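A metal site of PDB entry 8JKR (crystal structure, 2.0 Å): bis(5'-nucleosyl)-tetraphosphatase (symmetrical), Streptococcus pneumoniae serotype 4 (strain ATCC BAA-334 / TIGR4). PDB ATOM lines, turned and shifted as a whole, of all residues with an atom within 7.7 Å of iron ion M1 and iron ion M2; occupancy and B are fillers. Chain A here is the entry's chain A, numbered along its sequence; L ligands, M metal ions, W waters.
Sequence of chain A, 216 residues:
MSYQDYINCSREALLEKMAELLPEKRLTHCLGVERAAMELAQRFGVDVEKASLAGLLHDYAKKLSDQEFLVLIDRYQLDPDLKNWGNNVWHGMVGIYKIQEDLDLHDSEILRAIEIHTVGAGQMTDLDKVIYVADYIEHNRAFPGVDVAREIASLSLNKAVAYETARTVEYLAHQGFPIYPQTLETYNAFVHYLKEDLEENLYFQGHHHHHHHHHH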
ATOM      1  N   ARG A  26       0.421  23.525  16.566  1.00  0.00           N
ATOM      2  CA  ARG A  26      -0.454  22.750  15.683  1.00  0.00           C
ATOM      3  C   ARG A  26      -1.301  23.653  14.758  1.00  0.00           C
ATOM      4  O   ARG A  26      -1.497  23.340  13.565  1.00  0.00           O
ATOM      5  CB  ARG A  26      -1.327  21.777  16.510  1.00  0.00           C
ATOM      6  CG  ARG A  26      -2.140  20.747  15.709  1.00  0.00           C
ATOM      7  CD  ARG A  26      -1.302  19.970  14.693  1.00  0.00           C
ATOM      8  NE  ARG A  26      -0.261  19.176  15.356  1.00  0.00           N
ATOM      9  CZ  ARG A  26       0.635  18.402  14.748  1.00  0.00           C
ATOM     10  NH1 ARG A  26       1.501  17.743  15.489  1.00  0.00           N
ATOM     11  NH2 ARG A  26       0.651  18.265  13.426  1.00  0.00           N
ATOM     12  N   HIS A  29       1.083  25.168  12.205  1.00  0.00           N
ATOM     13  CA  HIS A  29       1.251  24.080  11.218  1.00  0.00           C
ATOM     14  C   HIS A  29       0.112  24.102  10.198  1.00  0.00           C
ATOM     15  O   HIS A  29       0.358  24.129   9.000  1.00  0.00           O
ATOM     16  CB  HIS A  29       1.358  22.708  11.907  1.00  0.00           C
ATOM     17  CG  HIS A  29       1.184  21.528  10.987  1.00  0.00           C
ATOM     18  ND1 HIS A  29       2.102  21.225  10.003  1.00  0.00           N
ATOM     19  CD2 HIS A  29       0.217  20.584  10.911  1.00  0.00           C
ATOM     20  CE1 HIS A  29       1.715  20.132   9.367  1.00  0.00           C
ATOM     21  NE2 HIS A  29       0.575  19.723   9.888  1.00  0.00           N
ATOM     22  N   CYS A  30      -1.128  24.137  10.701  1.00  0.00           N
ATOM     23  CA  CYS A  30      -2.325  24.136   9.846  1.00  0.00           C
ATOM     24  C   CYS A  30      -2.346  25.347   8.912  1.00  0.00           C
ATOM     25  O   CYS A  30      -2.702  25.208   7.740  1.00  0.00           O
ATOM     26  CB  CYS A  30      -3.610  24.073  10.684  1.00  0.00           C
ATOM     27  SG  CYS A  30      -3.940  22.434  11.370  1.00  0.00           S
ATOM     28  N   VAL A  33       0.148  24.665   6.198  1.00  0.00           N
ATOM     29  CA  VAL A  33      -0.395  23.703   5.223  1.00  0.00           C
ATOM     30  C   VAL A  33      -1.397  24.390   4.307  1.00  0.00           C
ATOM     31  O   VAL A  33      -1.427  24.101   3.113  1.00  0.00           O
ATOM     32  CB  VAL A  33      -1.001  22.434   5.898  1.00  0.00           C
ATOM     33  CG1 VAL A  33      -1.601  21.460   4.882  1.00  0.00           C
ATOM     34  CG2 VAL A  33       0.082  21.680   6.697  1.00  0.00           C
ATOM     35  N   GLY A  55      -6.286  22.036   3.592  1.00  0.00           N
ATOM     36  CA  GLY A  55      -4.979  22.193   4.242  1.00  0.00           C
ATOM     37  C   GLY A  55      -5.071  22.810   5.622  1.00  0.00           C
ATOM     38  O   GLY A  55      -4.388  22.366   6.567  1.00  0.00           O
ATOM     39  N   HIS A  58      -6.890  20.013   7.811  1.00  0.00           N
ATOM     40  CA  HIS A  58      -6.491  18.605   7.793  1.00  0.00           C
ATOM     41  C   HIS A  58      -6.197  18.015   9.199  1.00  0.00           C
ATOM     42  O   HIS A  58      -6.499  16.846   9.447  1.00  0.00           O
ATOM     43  CB  HIS A  58      -5.317  18.383   6.854  1.00  0.00           C
ATOM     44  CG  HIS A  58      -4.011  18.746   7.483  1.00  0.00           C
ATOM     45  ND1 HIS A  58      -3.665  20.045   7.750  1.00  0.00           N
ATOM     46  CD2 HIS A  58      -3.011  17.975   7.964  1.00  0.00           C
ATOM     47  CE1 HIS A  58      -2.494  20.069   8.348  1.00  0.00           C
ATOM     48  NE2 HIS A  58      -2.074  18.828   8.474  1.00  0.00           N
ATOM     49  N   ASP A  59      -5.618  18.833  10.098  1.00  0.00           N
ATOM     50  CA  ASP A  59      -5.314  18.412  11.468  1.00  0.00           C
ATOM     51  C   ASP A  59      -6.271  18.960  12.529  1.00  0.00           C
ATOM     52  O   ASP A  59      -5.924  19.028  13.701  1.00  0.00           O
ATOM     53  CB  ASP A  59      -3.873  18.734  11.853  1.00  0.00           C
ATOM     54  CG  ASP A  59      -2.892  17.662  11.410  1.00  0.00           C
ATOM     55  OD1 ASP A  59      -3.324  16.562  11.015  1.00  0.00           O
ATOM     56  OD2 ASP A  59      -1.685  17.948  11.414  1.00  0.00           O
ATOM     57  N   TYR A  60      -7.468  19.336  12.095  1.00  0.00           N
ATOM     58  CA  TYR A  60      -8.514  19.897  12.964  1.00  0.00           C
ATOM     59  C   TYR A  60      -8.778  18.993  14.177  1.00  0.00           C
ATOM     60  O   TYR A  60      -8.781  19.462  15.314  1.00  0.00           O
ATOM     61  CB  TYR A  60      -9.786  20.067  12.140  1.00  0.00           C
ATOM     62  CG  TYR A  60     -10.996  20.626  12.876  1.00  0.00           C
ATOM     63  CD1 TYR A  60     -11.874  19.781  13.562  1.00  0.00           C
ATOM     64  CD2 TYR A  60     -11.288  22.001  12.817  1.00  0.00           C
ATOM     65  CE1 TYR A  60     -13.004  20.285  14.208  1.00  0.00           C
ATOM     66  CE2 TYR A  60     -12.408  22.525  13.462  1.00  0.00           C
ATOM     67  CZ  TYR A  60     -13.267  21.654  14.144  1.00  0.00           C
ATOM     68  OH  TYR A  60     -14.360  22.159  14.782  1.00  0.00           O
ATOM     69  N   LYS A  62      -6.954  16.696  15.486  1.00  0.00           N
ATOM     70  CA  LYS A  62      -5.685  16.165  15.996  1.00  0.00           C
ATOM     71  C   LYS A  62      -5.736  15.803  17.476  1.00  0.00           C
ATOM     72  O   LYS A  62      -5.176  14.774  17.888  1.00  0.00           O
ATOM     73  CB  LYS A  62      -4.546  17.161  15.727  1.00  0.00           C
ATOM     74  CG  LYS A  62      -3.133  16.695  16.072  1.00  0.00           C
ATOM     75  CD  LYS A  62      -2.636  15.522  15.226  1.00  0.00           C
ATOM     76  CE  LYS A  62      -1.140  15.353  15.388  1.00  0.00           C
ATOM     77  NZ  LYS A  62      -0.640  14.149  14.671  1.00  0.00           N
ATOM     78  N   ASN A  87      -4.488   7.534  17.432  1.00  0.00           N
ATOM     79  CA  ASN A  87      -4.602   8.918  16.946  1.00  0.00           C
ATOM     80  C   ASN A  87      -4.066   9.132  15.522  1.00  0.00           C
ATOM     81  O   ASN A  87      -4.742   9.749  14.695  1.00  0.00           O
ATOM     82  CB  ASN A  87      -3.930   9.903  17.927  1.00  0.00           C
ATOM     83  CG  ASN A  87      -4.215  11.362  17.584  1.00  0.00           C
ATOM     84  OD1 ASN A  87      -3.575  11.945  16.710  1.00  0.00           O
ATOM     85  ND2 ASN A  87      -5.164  11.967  18.296  1.00  0.00           N
ATOM     86  N   ASN A  88      -2.865   8.612  15.240  1.00  0.00           N
ATOM     87  CA  ASN A  88      -2.224   8.762  13.930  1.00  0.00           C
ATOM     88  C   ASN A  88      -3.126   8.413  12.768  1.00  0.00           C
ATOM     89  O   ASN A  88      -3.248   9.195  11.812  1.00  0.00           O
ATOM     90  CB  ASN A  88      -0.928   7.935  13.861  1.00  0.00           C
ATOM     91  CG  ASN A  88       0.162   8.522  14.736  1.00  0.00           C
ATOM     92  OD1 ASN A  88      -0.009   9.583  15.303  1.00  0.00           O
ATOM     93  ND2 ASN A  88       1.294   7.856  14.802  1.00  0.00           N
ATOM     94  N   HIS A  91      -7.207  10.567  13.349  1.00  0.00           N
ATOM     95  CA  HIS A  91      -7.435  12.027  13.252  1.00  0.00           C
ATOM     96  C   HIS A  91      -7.883  12.486  11.864  1.00  0.00           C
ATOM     97  O   HIS A  91      -8.713  13.396  11.740  1.00  0.00           O
ATOM     98  CB  HIS A  91      -6.279  12.851  13.870  1.00  0.00           C
ATOM     99  CG  HIS A  91      -5.055  12.980  13.009  1.00  0.00           C
ATOM    100  ND1 HIS A  91      -4.088  11.995  12.928  1.00  0.00           N
ATOM    101  CD2 HIS A  91      -4.616  14.010  12.252  1.00  0.00           C
ATOM    102  CE1 HIS A  91      -3.113  12.412  12.138  1.00  0.00           C
ATOM    103  NE2 HIS A  91      -3.413  13.623  11.710  1.00  0.00           N
ATOM    104  N   GLY A  92      -7.372  11.808  10.824  1.00  0.00           N
ATOM    105  CA  GLY A  92      -7.848  12.021   9.473  1.00  0.00           C
ATOM    106  C   GLY A  92      -8.983  11.083   9.154  1.00  0.00           C
ATOM    107  O   GLY A  92     -10.051  11.529   8.760  1.00  0.00           O
ATOM    108  N   ILE A 114      -8.787  15.213   3.432  1.00  0.00           N
ATOM    109  CA  ILE A 114      -8.536  15.187   4.876  1.00  0.00           C
ATOM    110  C   ILE A 114      -8.443  13.724   5.389  1.00  0.00           C
ATOM    111  O   ILE A 114      -7.507  13.386   6.120  1.00  0.00           O
ATOM    112  CB  ILE A 114      -9.583  16.018   5.680  1.00  0.00           C
ATOM    113  CG1 ILE A 114      -9.550  17.498   5.231  1.00  0.00           C
ATOM    114  CG2 ILE A 114      -9.285  15.938   7.179  1.00  0.00           C
ATOM    115  CD1 ILE A 114     -10.562  18.402   5.919  1.00  0.00           C
ATOM    116  N   HIS A 117      -4.994  11.994   4.583  1.00  0.00           N
ATOM    117  CA  HIS A 117      -3.803  12.843   4.587  1.00  0.00           C
ATOM    118  C   HIS A 117      -2.588  12.207   5.275  1.00  0.00           C
ATOM    119  O   HIS A 117      -1.463  12.563   4.970  1.00  0.00           O
ATOM    120  CB  HIS A 117      -4.073  14.244   5.158  1.00  0.00           C
ATOM    121  CG  HIS A 117      -4.076  14.306   6.652  1.00  0.00           C
ATOM    122  ND1 HIS A 117      -5.239  14.150   7.394  1.00  0.00           N
ATOM    123  CD2 HIS A 117      -3.089  14.533   7.545  1.00  0.00           C
ATOM    124  CE1 HIS A 117      -4.951  14.274   8.680  1.00  0.00           C
ATOM    125  NE2 HIS A 117      -3.661  14.507   8.801  1.00  0.00           N
ATOM    126  N   THR A 118      -2.831  11.284   6.195  1.00  0.00           N
ATOM    127  CA  THR A 118      -1.749  10.610   6.945  1.00  0.00           C
ATOM    128  C   THR A 118      -1.248   9.355   6.227  1.00  0.00           C
ATOM    129  O   THR A 118      -0.043   9.139   6.128  1.00  0.00           O
ATOM    130  CB  THR A 118      -2.219  10.230   8.365  1.00  0.00           C
ATOM    131  OG1 THR A 118      -2.729  11.391   9.030  1.00  0.00           O
ATOM    132  CG2 THR A 118      -1.112   9.600   9.180  1.00  0.00           C
ATOM    133  N   ILE A 131      -2.713  17.837  -0.530  1.00  0.00           N
ATOM    134  CA  ILE A 131      -2.810  17.927   0.951  1.00  0.00           C
ATOM    135  C   ILE A 131      -1.722  17.032   1.589  1.00  0.00           C
ATOM    136  O   ILE A 131      -1.001  17.464   2.497  1.00  0.00           O
ATOM    137  CB  ILE A 131      -4.235  17.564   1.449  1.00  0.00           C
ATOM    138  CG1 ILE A 131      -5.270  18.507   0.806  1.00  0.00           C
ATOM    139  CG2 ILE A 131      -4.351  17.616   2.978  1.00  0.00           C
ATOM    140  CD1 ILE A 131      -4.855  19.982   0.835  1.00  0.00           C
ATOM    141  N   ALA A 134       1.592  18.894   0.934  1.00  0.00           N
ATOM    142  CA  ALA A 134       1.615  20.193   1.615  1.00  0.00           C
ATOM    143  C   ALA A 134       1.853  20.053   3.108  1.00  0.00           C
ATOM    144  O   ALA A 134       2.546  20.870   3.715  1.00  0.00           O
ATOM    145  CB  ALA A 134       0.304  20.943   1.385  1.00  0.00           C
ATOM    146  N   ASP A 135       1.257  19.027   3.683  1.00  0.00           N
ATOM    147  CA  ASP A 135       1.404  18.669   5.093  1.00  0.00           C
ATOM    148  C   ASP A 135       2.890  18.499   5.456  1.00  0.00           C
ATOM    149  O   ASP A 135       3.381  18.975   6.496  1.00  0.00           O
ATOM    150  CB  ASP A 135       0.606  17.381   5.357  1.00  0.00           C
ATOM    151  CG  ASP A 135       0.574  16.987   6.819  1.00  0.00           C
ATOM    152  OD1 ASP A 135       0.711  17.862   7.688  1.00  0.00           O
ATOM    153  OD2 ASP A 135       0.409  15.774   7.088  1.00  0.00           O
ATOM    154  N   TYR A 136       3.609  17.873   4.527  1.00  0.00           N
ATOM    155  CA  TYR A 136       5.003  17.460   4.709  1.00  0.00           C
ATOM    156  C   TYR A 136       5.973  18.601   4.482  1.00  0.00           C
ATOM    157  O   TYR A 136       7.021  18.624   5.110  1.00  0.00           O
ATOM    158  CB  TYR A 136       5.291  16.349   3.710  1.00  0.00           C
ATOM    159  CG  TYR A 136       6.469  15.433   4.018  1.00  0.00           C
ATOM    160  CD1 TYR A 136       6.520  14.693   5.217  1.00  0.00           C
ATOM    161  CD2 TYR A 136       7.499  15.256   3.074  1.00  0.00           C
ATOM    162  CE1 TYR A 136       7.564  13.824   5.480  1.00  0.00           C
ATOM    163  CE2 TYR A 136       8.560  14.384   3.338  1.00  0.00           C
ATOM    164  CZ  TYR A 136       8.583  13.672   4.524  1.00  0.00           C
ATOM    165  OH  TYR A 136       9.638  12.818   4.773  1.00  0.00           O
ATOM    166  N   GLU A 138       5.270  22.105   4.440  1.00  0.00           N
ATOM    167  CA  GLU A 138       4.843  23.447   4.919  1.00  0.00           C
ATOM    168  C   GLU A 138       5.992  24.128   5.645  1.00  0.00           C
ATOM    169  O   GLU A 138       6.769  23.453   6.360  1.00  0.00           O
ATOM    170  CB  GLU A 138       3.540  23.398   5.736  1.00  0.00           C
ATOM    171  CG  GLU A 138       3.615  22.624   7.043  1.00  0.00           C
ATOM    172  CD  GLU A 138       3.998  23.487   8.252  1.00  0.00           C
ATOM    173  OE1 GLU A 138       4.253  24.705   8.098  1.00  0.00           O
ATOM    174  OE2 GLU A 138       4.021  22.929   9.370  1.00  0.00           O
ATOM    175  N   ARG A 141       8.039  23.365   8.924  1.00  0.00           N
ATOM    176  CA  ARG A 141       8.739  22.116   9.188  1.00  0.00           C
ATOM    177  C   ARG A 141      10.214  22.214   8.869  1.00  0.00           C
ATOM    178  O   ARG A 141      10.612  22.952   8.009  1.00  0.00           O
ATOM    179  CB  ARG A 141       8.045  20.992   8.476  1.00  0.00           C
ATOM    180  CG  ARG A 141       6.691  20.861   9.105  1.00  0.00           C
ATOM    181  CD  ARG A 141       5.998  19.619   8.700  1.00  0.00           C
ATOM    182  NE  ARG A 141       6.576  18.433   9.298  1.00  0.00           N
ATOM    183  CZ  ARG A 141       5.989  17.261   9.211  1.00  0.00           C
ATOM    184  NH1 ARG A 141       4.820  17.169   8.573  1.00  0.00           N
ATOM    185  NH2 ARG A 141       6.537  16.189   9.759  1.00  0.00           N
HETATM  186  N1  LIG L   1       1.996   7.416  10.887  1.00  0.00           N
HETATM  187  C1  LIG L   1       1.588   6.163  11.402  1.00  0.00           C
HETATM  188  N2  LIG L   1       1.158   5.196  10.586  1.00  0.00           N
HETATM  189  C2  LIG L   1       1.092   5.424   9.265  1.00  0.00           C
HETATM  190  C3  LIG L   1       1.500   6.666   8.724  1.00  0.00           C
HETATM  191  C4  LIG L   1       1.948   7.676   9.575  1.00  0.00           C
HETATM  192  O1  LIG L   1       1.649   5.953  12.638  1.00  0.00           O
HETATM  193  O2  LIG L   1       0.668   4.484   8.568  1.00  0.00           O
HETATM  194  C5  LIG L   1       2.505   8.437  11.789  1.00  0.00           C
HETATM  195  C6  LIG L   1       3.556   9.319  11.112  1.00  0.00           C
HETATM  196  O3  LIG L   1       4.856   9.003  11.598  1.00  0.00           O
HETATM  197  C7  LIG L   1       3.131  10.725  11.478  1.00  0.00           C
HETATM  198  C8  LIG L   1       1.842  10.612  12.262  1.00  0.00           C
HETATM  199  O4  LIG L   1       4.058  11.382  12.351  1.00  0.00           O
HETATM  200  O5  LIG L   1       1.429   9.243  12.256  1.00  0.00           O
HETATM  201  C9  LIG L   1       0.735  11.538  11.757  1.00  0.00           C
HETATM  202  O6  LIG L   1       0.937  11.735  10.367  1.00  0.00           O
HETATM  203  P1  LIG L   1       0.559  13.088   9.621  1.00  0.00           P
HETATM  204  O7  LIG L   1      -0.947  13.061   9.778  1.00  0.00           O
HETATM  205  O8  LIG L   1       1.366  14.095  10.386  1.00  0.00           O
HETATM  206  O9  LIG L   1       1.095  12.871   8.225  1.00  0.00           O
HETATM  207 FE    FE M   1      -0.389  17.970   9.543  1.00  0.00          FE
HETATM  208 FE    FE M   2      -2.195  14.833  10.351  1.00  0.00          FE
HETATM  209  O   HOH W   1      -0.876  15.331  11.801  1.00  0.00           O
HETATM  210  O   HOH W   2      -0.904  16.126   9.482  1.00  0.00           O
HETATM  211  O   HOH W   3       1.349  17.090  10.405  1.00  0.00           O
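Iron ion M1 is bound by water W2 (1.9 Å), a ring nitrogen (NE2) of His 29 (2.0 Å), water W3 (2.1 Å), the side-chain carboxylate of Asp 135 (2.2 Å), a ring nitrogen (NE2) of His 58 (2.2 Å) and the side-chain carboxylate of Asp 59 (2.3 Å).
Four residues have an atom within 4 Å of iron ion M1: His 29, His 58, Asp 59 and Asp 135.
The guanidinium group of Arg 141 sits at hydrogen-bond distance from the backbone carbonyl oxygen of Asp 135 (3.1 Å).
A ring nitrogen (ND1) of His 91 lies within hydrogen-bond range of the backbone carbonyl oxygen of Asn 88 (3.1 Å).
The side-chain hydroxyl (OG1) of Thr 118 sits close to a ring nitrogen (NE2) of His 117, at 3.3 Å.
A ring nitrogen (ND1) of His 29 is in hydrogen-bond range of the side-chain carboxylate (OE2) of Glu 138, 2.6 Å away.
A ring nitrogen (ND1) of His 58 sits at hydrogen-bond distance from the backbone carbonyl oxygen of Gly 55 (2.7 Å).
ND1 of His 91 lies within hydrogen-bond range of O of Asn 87.
The side-chain carboxylate (OD2) of Asp 59 sits close to the guanidinium group (NH2) of Arg 26 (3.1 Å).
A ring nitrogen (ND1) of His 117 lies within hydrogen-bond range of the backbone carbonyl oxygen (O) of Ile 114 (2.7 Å).
Iron ion M2 is bound by water W1 (2.0 Å), water W2 (2.0 Å), a ring nitrogen (NE2) of His 117 (2.2 Å), the side-chain carboxylate of Asp 59 (2.2 Å), a ring nitrogen (NE2) of His 91 (2.2 Å) and an oxygen (O7) of the ligand (2.2 Å).
Thr 118 touches iron ion M2.
Within 4 Å of iron ion M2: Asp 59, His 91, His 117 and Thr 118.
Water W3 lies within hydrogen-bond range of O8 of the ligand and NH2 of Arg 26.
Water W2 lies within hydrogen-bond range of OD2 of Asp 135 (2.8 Å) and O8 of the ligand (3.2 Å).
Water W1 lies within hydrogen-bond range of O8 of the ligand and NZ of Lys 62.
An oxygen (O5) of the ligand sits close to the side-chain amide nitrogen of Asn 88, at 2.9 Å.
The side-chain hydroxyl (OG1) of Thr 118 lies close to an oxygen (O7) of the ligand, 2.6 Å away.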
